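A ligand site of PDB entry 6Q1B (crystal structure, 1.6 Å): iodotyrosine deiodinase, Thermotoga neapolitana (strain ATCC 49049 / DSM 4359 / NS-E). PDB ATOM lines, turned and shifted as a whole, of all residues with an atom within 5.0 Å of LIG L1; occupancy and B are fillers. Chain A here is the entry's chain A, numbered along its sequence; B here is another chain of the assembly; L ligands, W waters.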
ATOM      1  N   ARG A  15       9.622  18.722 -19.501  1.00  0.00           N
ATOM      2  CA  ARG A  15      10.253  18.393 -20.755  1.00  0.00           C
ATOM      3  C   ARG A  15      11.057  19.545 -21.286  1.00  0.00           C
ATOM      4  O   ARG A  15      11.667  19.443 -22.368  1.00  0.00           O
ATOM      5  CB  ARG A  15       9.225  17.987 -21.789  1.00  0.00           C
ATOM      6  CG  ARG A  15       8.483  16.748 -21.385  1.00  0.00           C
ATOM      7  CD  ARG A  15       7.546  16.297 -22.454  1.00  0.00           C
ATOM      8  NE  ARG A  15       6.807  15.103 -22.074  1.00  0.00           N
ATOM      9  CZ  ARG A  15       5.630  15.100 -21.445  1.00  0.00           C
ATOM     10  NH1 ARG A  15       5.042  16.233 -21.088  1.00  0.00           N
ATOM     11  NH2 ARG A  15       5.047  13.960 -21.146  1.00  0.00           N
ATOM     12  N   GLU A  68      11.372   6.636 -31.808  1.00  0.00           N
ATOM     13  CA  GLU A  68      10.127   7.372 -31.692  1.00  0.00           C
ATOM     14  C   GLU A  68       9.523   7.650 -33.038  1.00  0.00           C
ATOM     15  O   GLU A  68       8.334   7.488 -33.245  1.00  0.00           O
ATOM     16  CB  GLU A  68      10.309   8.706 -30.975  1.00  0.00           C
ATOM     17  CG  GLU A  68      10.671   8.555 -29.521  1.00  0.00           C
ATOM     18  CD  GLU A  68       9.587   7.934 -28.683  1.00  0.00           C
ATOM     19  OE1 GLU A  68       8.542   7.477 -29.223  1.00  0.00           O
ATOM     20  OE2 GLU A  68       9.792   7.900 -27.448  1.00  0.00           O
ATOM     21  N   PHE A  71       7.829   4.773 -34.257  1.00  0.00           N
ATOM     22  CA  PHE A  71       6.700   4.509 -33.393  1.00  0.00           C
ATOM     23  C   PHE A  71       5.556   5.445 -33.744  1.00  0.00           C
ATOM     24  O   PHE A  71       4.409   5.012 -33.797  1.00  0.00           O
ATOM     25  CB  PHE A  71       7.108   4.647 -31.928  1.00  0.00           C
ATOM     26  CG  PHE A  71       5.963   4.912 -31.010  1.00  0.00           C
ATOM     27  CD1 PHE A  71       5.236   3.866 -30.475  1.00  0.00           C
ATOM     28  CD2 PHE A  71       5.597   6.202 -30.698  1.00  0.00           C
ATOM     29  CE1 PHE A  71       4.192   4.114 -29.641  1.00  0.00           C
ATOM     30  CE2 PHE A  71       4.548   6.441 -29.864  1.00  0.00           C
ATOM     31  CZ  PHE A  71       3.835   5.409 -29.338  1.00  0.00           C
ATOM     32  N   TYR A  72       5.876   6.700 -34.012  1.00  0.00           N
ATOM     33  CA  TYR A  72       4.840   7.674 -34.368  1.00  0.00           C
ATOM     34  C   TYR A  72       4.203   7.362 -35.693  1.00  0.00           C
ATOM     35  O   TYR A  72       3.047   7.696 -35.926  1.00  0.00           O
ATOM     36  CB  TYR A  72       5.413   9.083 -34.376  1.00  0.00           C
ATOM     37  CG  TYR A  72       5.313   9.674 -32.992  1.00  0.00           C
ATOM     38  CD1 TYR A  72       6.287   9.419 -32.028  1.00  0.00           C
ATOM     39  CD2 TYR A  72       4.194  10.407 -32.628  1.00  0.00           C
ATOM     40  CE1 TYR A  72       6.158   9.932 -30.772  1.00  0.00           C
ATOM     41  CE2 TYR A  72       4.064  10.909 -31.380  1.00  0.00           C
ATOM     42  CZ  TYR A  72       5.024  10.661 -30.448  1.00  0.00           C
ATOM     43  OH  TYR A  72       4.875  11.175 -29.202  1.00  0.00           O
ATOM     44  N   LEU A  79      -3.271   5.705 -27.400  1.00  0.00           N
ATOM     45  CA  LEU A  79      -2.008   6.385 -27.219  1.00  0.00           C
ATOM     46  C   LEU A  79      -1.784   7.356 -28.370  1.00  0.00           C
ATOM     47  O   LEU A  79      -1.401   8.510 -28.146  1.00  0.00           O
ATOM     48  CB  LEU A  79      -0.854   5.393 -27.112  1.00  0.00           C
ATOM     49  CG  LEU A  79       0.512   6.046 -26.906  1.00  0.00           C
ATOM     50  CD1 LEU A  79       0.529   6.985 -25.704  1.00  0.00           C
ATOM     51  CD2 LEU A  79       1.550   4.962 -26.711  1.00  0.00           C
ATOM     52  N   TRP A  82      -3.982  10.320 -27.859  1.00  0.00           N
ATOM     53  CA  TRP A  82      -3.523  11.149 -26.787  1.00  0.00           C
ATOM     54  C   TRP A  82      -2.310  11.943 -27.223  1.00  0.00           C
ATOM     55  O   TRP A  82      -2.213  13.134 -26.965  1.00  0.00           O
ATOM     56  CB  TRP A  82      -3.181  10.265 -25.594  1.00  0.00           C
ATOM     57  CG  TRP A  82      -2.804  11.006 -24.361  1.00  0.00           C
ATOM     58  CD1 TRP A  82      -3.648  11.496 -23.425  1.00  0.00           C
ATOM     59  CD2 TRP A  82      -1.490  11.330 -23.936  1.00  0.00           C
ATOM     60  NE1 TRP A  82      -2.948  12.116 -22.434  1.00  0.00           N
ATOM     61  CE2 TRP A  82      -1.615  12.016 -22.710  1.00  0.00           C
ATOM     62  CE3 TRP A  82      -0.220  11.113 -24.461  1.00  0.00           C
ATOM     63  CZ2 TRP A  82      -0.523  12.483 -22.012  1.00  0.00           C
ATOM     64  CZ3 TRP A  82       0.881  11.562 -23.752  1.00  0.00           C
ATOM     65  CH2 TRP A  82       0.712  12.252 -22.538  1.00  0.00           C
ATOM     66  N   LEU A  83      -1.365  11.278 -27.867  1.00  0.00           N
ATOM     67  CA  LEU A  83      -0.162  11.949 -28.339  1.00  0.00           C
ATOM     68  C   LEU A  83      -0.517  13.009 -29.338  1.00  0.00           C
ATOM     69  O   LEU A  83       0.037  14.101 -29.301  1.00  0.00           O
ATOM     70  CB  LEU A  83       0.810  10.962 -28.971  1.00  0.00           C
ATOM     71  CG  LEU A  83       1.387   9.953 -27.995  1.00  0.00           C
ATOM     72  CD1 LEU A  83       2.141   8.897 -28.805  1.00  0.00           C
ATOM     73  CD2 LEU A  83       2.278  10.654 -26.994  1.00  0.00           C
ATOM     74  N   PHE A  88       2.397  15.806 -29.281  1.00  0.00           N
ATOM     75  CA  PHE A  88       3.675  15.137 -29.147  1.00  0.00           C
ATOM     76  C   PHE A  88       4.251  14.793 -30.493  1.00  0.00           C
ATOM     77  O   PHE A  88       3.512  14.539 -31.458  1.00  0.00           O
ATOM     78  CB  PHE A  88       3.527  13.844 -28.354  1.00  0.00           C
ATOM     79  CG  PHE A  88       3.464  14.038 -26.882  1.00  0.00           C
ATOM     80  CD1 PHE A  88       2.383  14.621 -26.290  1.00  0.00           C
ATOM     81  CD2 PHE A  88       4.486  13.609 -26.082  1.00  0.00           C
ATOM     82  CE1 PHE A  88       2.323  14.789 -24.924  1.00  0.00           C
ATOM     83  CE2 PHE A  88       4.429  13.762 -24.734  1.00  0.00           C
ATOM     84  CZ  PHE A  88       3.367  14.357 -24.159  1.00  0.00           C
ATOM     85  N   THR A  89       5.572  14.740 -30.570  1.00  0.00           N
ATOM     86  CA  THR A  89       6.180  14.203 -31.757  1.00  0.00           C
ATOM     87  C   THR A  89       7.361  13.387 -31.334  1.00  0.00           C
ATOM     88  O   THR A  89       7.645  13.244 -30.153  1.00  0.00           O
ATOM     89  CB  THR A  89       6.652  15.281 -32.740  1.00  0.00           C
ATOM     90  OG1 THR A  89       7.830  15.914 -32.238  1.00  0.00           O
ATOM     91  CG2 THR A  89       5.588  16.287 -32.946  1.00  0.00           C
ATOM     92  N   LYS A  92      12.861  14.644 -29.470  1.00  0.00           N
ATOM     93  CA  LYS A  92      13.056  14.631 -28.026  1.00  0.00           C
ATOM     94  C   LYS A  92      14.212  15.511 -27.649  1.00  0.00           C
ATOM     95  O   LYS A  92      15.241  15.036 -27.178  1.00  0.00           O
ATOM     96  CB  LYS A  92      13.300  13.207 -27.543  1.00  0.00           C
ATOM     97  CG  LYS A  92      12.201  12.258 -27.905  1.00  0.00           C
ATOM     98  CD  LYS A  92      10.840  12.662 -27.300  1.00  0.00           C
ATOM     99  CE  LYS A  92       9.701  11.967 -27.972  1.00  0.00           C
ATOM    100  NZ  LYS A  92       8.392  12.616 -27.662  1.00  0.00           N
ATOM    101  N   TYR A 138      11.098   9.069 -19.372  1.00  0.00           N
ATOM    102  CA  TYR A 138      11.082   8.948 -20.801  1.00  0.00           C
ATOM    103  C   TYR A 138      11.348   7.508 -21.160  1.00  0.00           C
ATOM    104  O   TYR A 138      12.334   6.930 -20.735  1.00  0.00           O
ATOM    105  CB  TYR A 138      12.084   9.869 -21.451  1.00  0.00           C
ATOM    106  CG  TYR A 138      12.140   9.574 -22.905  1.00  0.00           C
ATOM    107  CD1 TYR A 138      11.024   9.755 -23.707  1.00  0.00           C
ATOM    108  CD2 TYR A 138      13.271   9.030 -23.474  1.00  0.00           C
ATOM    109  CE1 TYR A 138      11.048   9.423 -25.025  1.00  0.00           C
ATOM    110  CE2 TYR A 138      13.310   8.690 -24.783  1.00  0.00           C
ATOM    111  CZ  TYR A 138      12.201   8.902 -25.568  1.00  0.00           C
ATOM    112  OH  TYR A 138      12.232   8.566 -26.882  1.00  0.00           O
ATOM    113  N   THR A 139      10.479   6.949 -21.986  1.00  0.00           N
ATOM    114  CA  THR A 139      10.537   5.555 -22.335  1.00  0.00           C
ATOM    115  C   THR A 139      10.434   5.463 -23.850  1.00  0.00           C
ATOM    116  O   THR A 139       9.338   5.495 -24.398  1.00  0.00           O
ATOM    117  CB  THR A 139       9.412   4.768 -21.684  1.00  0.00           C
ATOM    118  OG1 THR A 139       8.170   5.388 -21.992  1.00  0.00           O
ATOM    119  CG2 THR A 139       9.577   4.740 -20.168  1.00  0.00           C
ATOM    120  N   PRO A 140      11.573   5.406 -24.537  1.00  0.00           N
ATOM    121  CA  PRO A 140      11.548   5.243 -25.991  1.00  0.00           C
ATOM    122  C   PRO A 140      10.991   3.877 -26.326  1.00  0.00           C
ATOM    123  O   PRO A 140      10.993   2.997 -25.464  1.00  0.00           O
ATOM    124  CB  PRO A 140      13.007   5.358 -26.379  1.00  0.00           C
ATOM    125  CG  PRO A 140      13.744   4.877 -25.169  1.00  0.00           C
ATOM    126  CD  PRO A 140      12.937   5.337 -23.997  1.00  0.00           C
ATOM    127  N   SER B  39       1.973   8.994 -15.106  1.00  0.00           N
ATOM    128  CA  SER B  39       1.700   7.719 -15.678  1.00  0.00           C
ATOM    129  C   SER B  39       1.802   7.842 -17.162  1.00  0.00           C
ATOM    130  O   SER B  39       1.687   8.937 -17.708  1.00  0.00           O
ATOM    131  CB  SER B  39       0.328   7.198 -15.280  1.00  0.00           C
ATOM    132  OG  SER B  39      -0.692   8.079 -15.702  1.00  0.00           O
ATOM    133  N   GLY B  40       2.027   6.716 -17.815  1.00  0.00           N
ATOM    134  CA  GLY B  40       2.083   6.703 -19.255  1.00  0.00           C
ATOM    135  C   GLY B  40       0.775   7.254 -19.806  1.00  0.00           C
ATOM    136  O   GLY B  40      -0.306   6.859 -19.387  1.00  0.00           O
ATOM    137  N   MET B  41       0.918   8.160 -20.756  1.00  0.00           N
ATOM    138  CA  MET B  41      -0.167   8.936 -21.374  1.00  0.00           C
ATOM    139  C   MET B  41      -1.194   9.447 -20.372  1.00  0.00           C
ATOM    140  O   MET B  41      -2.360   9.691 -20.709  1.00  0.00           O
ATOM    141  CB  MET B  41      -0.839   8.133 -22.489  1.00  0.00           C
ATOM    142  CG  MET B  41      -1.663   6.944 -22.119  1.00  0.00           C
ATOM    143  SD  MET B  41      -2.687   6.505 -23.546  1.00  0.00           S
ATOM    144  CE  MET B  41      -4.029   7.666 -23.347  1.00  0.00           C
ATOM    145  N   ASN B  42      -0.703   9.729 -19.156  1.00  0.00           N
ATOM    146  CA  ASN B  42      -1.513  10.202 -18.048  1.00  0.00           C
ATOM    147  C   ASN B  42      -2.766   9.368 -17.885  1.00  0.00           C
ATOM    148  O   ASN B  42      -3.832   9.857 -17.498  1.00  0.00           O
ATOM    149  CB  ASN B  42      -1.889  11.665 -18.225  1.00  0.00           C
ATOM    150  CG  ASN B  42      -2.463  12.265 -16.972  1.00  0.00           C
ATOM    151  OD1 ASN B  42      -2.060  11.929 -15.879  1.00  0.00           O
ATOM    152  ND2 ASN B  42      -3.449  13.129 -17.141  1.00  0.00           N
ATOM    153  N   PRO B 111      -0.821   2.284 -21.593  1.00  0.00           N
ATOM    154  CA  PRO B 111       0.610   2.242 -21.863  1.00  0.00           C
ATOM    155  C   PRO B 111       1.416   2.367 -20.593  1.00  0.00           C
ATOM    156  O   PRO B 111       1.160   3.244 -19.759  1.00  0.00           O
ATOM    157  CB  PRO B 111       0.849   3.466 -22.752  1.00  0.00           C
ATOM    158  CG  PRO B 111      -0.454   3.802 -23.301  1.00  0.00           C
ATOM    159  CD  PRO B 111      -1.469   3.401 -22.291  1.00  0.00           C
ATOM    160  N   TYR B 112       2.417   1.504 -20.463  1.00  0.00           N
ATOM    161  CA  TYR B 112       3.298   1.497 -19.322  1.00  0.00           C
ATOM    162  C   TYR B 112       2.487   1.480 -18.034  1.00  0.00           C
ATOM    163  O   TYR B 112       2.853   2.129 -17.043  1.00  0.00           O
ATOM    164  CB  TYR B 112       4.213   2.706 -19.353  1.00  0.00           C
ATOM    165  CG  TYR B 112       4.885   2.926 -20.694  1.00  0.00           C
ATOM    166  CD1 TYR B 112       5.922   2.114 -21.108  1.00  0.00           C
ATOM    167  CD2 TYR B 112       4.485   3.958 -21.533  1.00  0.00           C
ATOM    168  CE1 TYR B 112       6.543   2.320 -22.329  1.00  0.00           C
ATOM    169  CE2 TYR B 112       5.093   4.160 -22.759  1.00  0.00           C
ATOM    170  CZ  TYR B 112       6.124   3.340 -23.151  1.00  0.00           C
ATOM    171  OH  TYR B 112       6.746   3.546 -24.372  1.00  0.00           O
HETATM  172  N1  LIG L   1       7.585   7.716 -25.829  1.00  0.00           N
HETATM  173  C1  LIG L   1       6.827   8.449 -26.805  1.00  0.00           C
HETATM  174  C2  LIG L   1       7.199   9.903 -26.637  1.00  0.00           C
HETATM  175  O1  LIG L   1       6.593  10.744 -27.481  1.00  0.00           O
HETATM  176  O2  LIG L   1       7.949  10.348 -25.774  1.00  0.00           O
HETATM  177  C3  LIG L   1       5.331   8.330 -26.585  1.00  0.00           C
HETATM  178  C4  LIG L   1       4.842   8.621 -25.215  1.00  0.00           C
HETATM  179  C5  LIG L   1       4.418   7.557 -24.409  1.00  0.00           C
HETATM  180  C6  LIG L   1       4.729   9.933 -24.740  1.00  0.00           C
HETATM  181  C7  LIG L   1       3.895   7.831 -23.143  1.00  0.00           C
HETATM  182  C8  LIG L   1       4.211  10.217 -23.474  1.00  0.00           C
HETATM  183  C9  LIG L   1       3.812   9.149 -22.667  1.00  0.00           C
HETATM  184  O3  LIG L   1       3.309   9.410 -21.444  1.00  0.00           O
HETATM  185  F1  LIG L   1       3.493   6.837 -22.327  1.00  0.00           F
HETATM  186  N1  LG2 L   2       6.435  11.350 -21.287  1.00  0.00           N
HETATM  187  C1  LG2 L   2       6.986  11.494 -22.500  1.00  0.00           C
HETATM  188  O1  LG2 L   2       7.025  12.613 -23.013  1.00  0.00           O
HETATM  189  N2  LG2 L   2       7.495  10.416 -23.168  1.00  0.00           N
HETATM  190  C2  LG2 L   2       7.485   9.162 -22.621  1.00  0.00           C
HETATM  191  O2  LG2 L   2       7.942   8.211 -23.240  1.00  0.00           O
HETATM  192  C3  LG2 L   2       6.911   9.009 -21.382  1.00  0.00           C
HETATM  193  N3  LG2 L   2       6.882   7.779 -20.805  1.00  0.00           N
HETATM  194  C4  LG2 L   2       6.368   7.649 -19.555  1.00  0.00           C
HETATM  195  C5  LG2 L   2       6.394   6.385 -18.988  1.00  0.00           C
HETATM  196  C6  LG2 L   2       5.881   6.207 -17.722  1.00  0.00           C
HETATM  197  C7  LG2 L   2       5.916   4.844 -17.118  1.00  0.00           C
HETATM  198  C8  LG2 L   2       5.353   7.297 -17.055  1.00  0.00           C
HETATM  199  C9  LG2 L   2       4.854   7.089 -15.657  1.00  0.00           C
HETATM  200  C10 LG2 L   2       5.341   8.575 -17.609  1.00  0.00           C
HETATM  201  C11 LG2 L   2       5.853   8.742 -18.883  1.00  0.00           C
HETATM  202  N4  LG2 L   2       5.849   9.992 -19.494  1.00  0.00           N
HETATM  203  C12 LG2 L   2       6.415  10.115 -20.727  1.00  0.00           C
HETATM  204  C13 LG2 L   2       5.307  11.196 -18.824  1.00  0.00           C
HETATM  205  C14 LG2 L   2       3.781  11.162 -18.900  1.00  0.00           C
HETATM  206  O3  LG2 L   2       3.360  11.599 -20.174  1.00  0.00           O
HETATM  207  C15 LG2 L   2       3.224  12.031 -17.772  1.00  0.00           C
HETATM  208  O4  LG2 L   2       3.554  11.449 -16.531  1.00  0.00           O
HETATM  209  C16 LG2 L   2       1.715  12.244 -17.872  1.00  0.00           C
HETATM  210  O5  LG2 L   2       1.495  13.005 -19.035  1.00  0.00           O
HETATM  211  C17 LG2 L   2       1.208  13.024 -16.679  1.00  0.00           C
HETATM  212  O6  LG2 L   2       1.954  14.210 -16.600  1.00  0.00           O
HETATM  213  P1  LG2 L   2       1.648  15.266 -15.455  1.00  0.00           P
HETATM  214  O7  LG2 L   2       2.470  16.527 -15.779  1.00  0.00           O
HETATM  215  O8  LG2 L   2       2.057  14.673 -14.102  1.00  0.00           O
HETATM  216  O9  LG2 L   2       0.137  15.504 -15.530  1.00  0.00           O
HETATM  217  O   HOH W   1       7.222   5.505 -27.929  1.00  0.00           O
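The backbone carbonyl oxygen (O) of Thr 139 sits at hydrogen-bond distance from a nitrogen (N1) of LIG L1, 3.2 Å away.
An oxygen (O4) of LG2 L2 sits close to the backbone carbonyl oxygen (O) of Ser 39 of chain B (3.3 Å).
A nitrogen (N3) of LG2 L2 lies within hydrogen-bond range of the side-chain hydroxyl (OG1) of Thr 139 (3.0 Å).
O1 of LG2 L2 sits at hydrogen-bond distance from NE of Arg 15 (2.7 Å).
O1 of LIG L1 is in hydrogen-bond range of OH of Tyr 72 (2.5 Å).
N of Thr 139 is in hydrogen-bond range of O2 of LG2 L2 (3.1 Å).
An oxygen (O1) of LIG L1 is in salt-bridge range of the side-chain amino group (NZ) of Lys 92, 2.6 Å away.
N of Ser 39 of chain B is in hydrogen-bond range of O4 of LG2 L2, at 3.2 Å.
O3 of LIG L1 sits at hydrogen-bond distance from N of Met 41 of chain B (2.8 Å).
A nitrogen (N1) of LIG L1 lies within salt-bridge range of the side-chain carboxylate of Glu 68 (2.7 Å).
An oxygen (O3) of LG2 L2 lies within hydrogen-bond range of an oxygen (O3) of LIG L1.
CE2 of Phe 71 touches C3 of LIG L1, at 3.9 Å.
Trp 82 touches LIG L1.
Leu 83 touches LIG L1 (CD2 to C6, 3.4 Å).
Phe 88 touches LIG L1.
Thr 89 touches LIG L1 (O to O1, 3.8 Å).
CE1 of Tyr 138 touches O2 of LIG L1, at 3.3 Å.
Gly 40 of chain B touches LIG L1 (CA to F1, 3.4 Å).
Tyr 112 of chain B touches LIG L1 (CD2 to F1, 3.1 Å).
Hydrophobic or aromatic side chains that line LIG L1: Phe 71, Tyr 72, Trp 82, Leu 83, Phe 88, Tyr 138 and Tyr 112 of chain B.
Within 4 Å of LIG L1: Glu 68, Phe 71, Tyr 72, Trp 82, Leu 83, Phe 88, Thr 89, Lys 92, Tyr 138, Thr 139, Gly 40 of chain B, Met 41 of chain B and Tyr 112 of chain B.
The nearest printed residue that does not touch LIG L1 is Ser 39 of chain B (4.1 Å).
NE1 of Trp 82 is in hydrogen-bond range of O of Met 41 of chain B.
OE2 of Glu 68 is in hydrogen-bond range of OH of Tyr 138, 2.6 Å away.
OH of Tyr 112 of chain B is in hydrogen-bond range of O of Thr 139 (3.2 Å).
The backbone NH (N) of Phe 88 lies within hydrogen-bond range of the backbone carbonyl oxygen (O) of Leu 83 (2.9 Å).
The backbone carbonyl oxygen of Thr 89 is in hydrogen-bond range of the side-chain amino group of Lys 92 (2.7 Å).
Water W1 bridges the side-chain carboxylate (OE1) of Glu 68 (2.7 Å) and a nitrogen (N1) of LIG L1 (3.1 Å).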
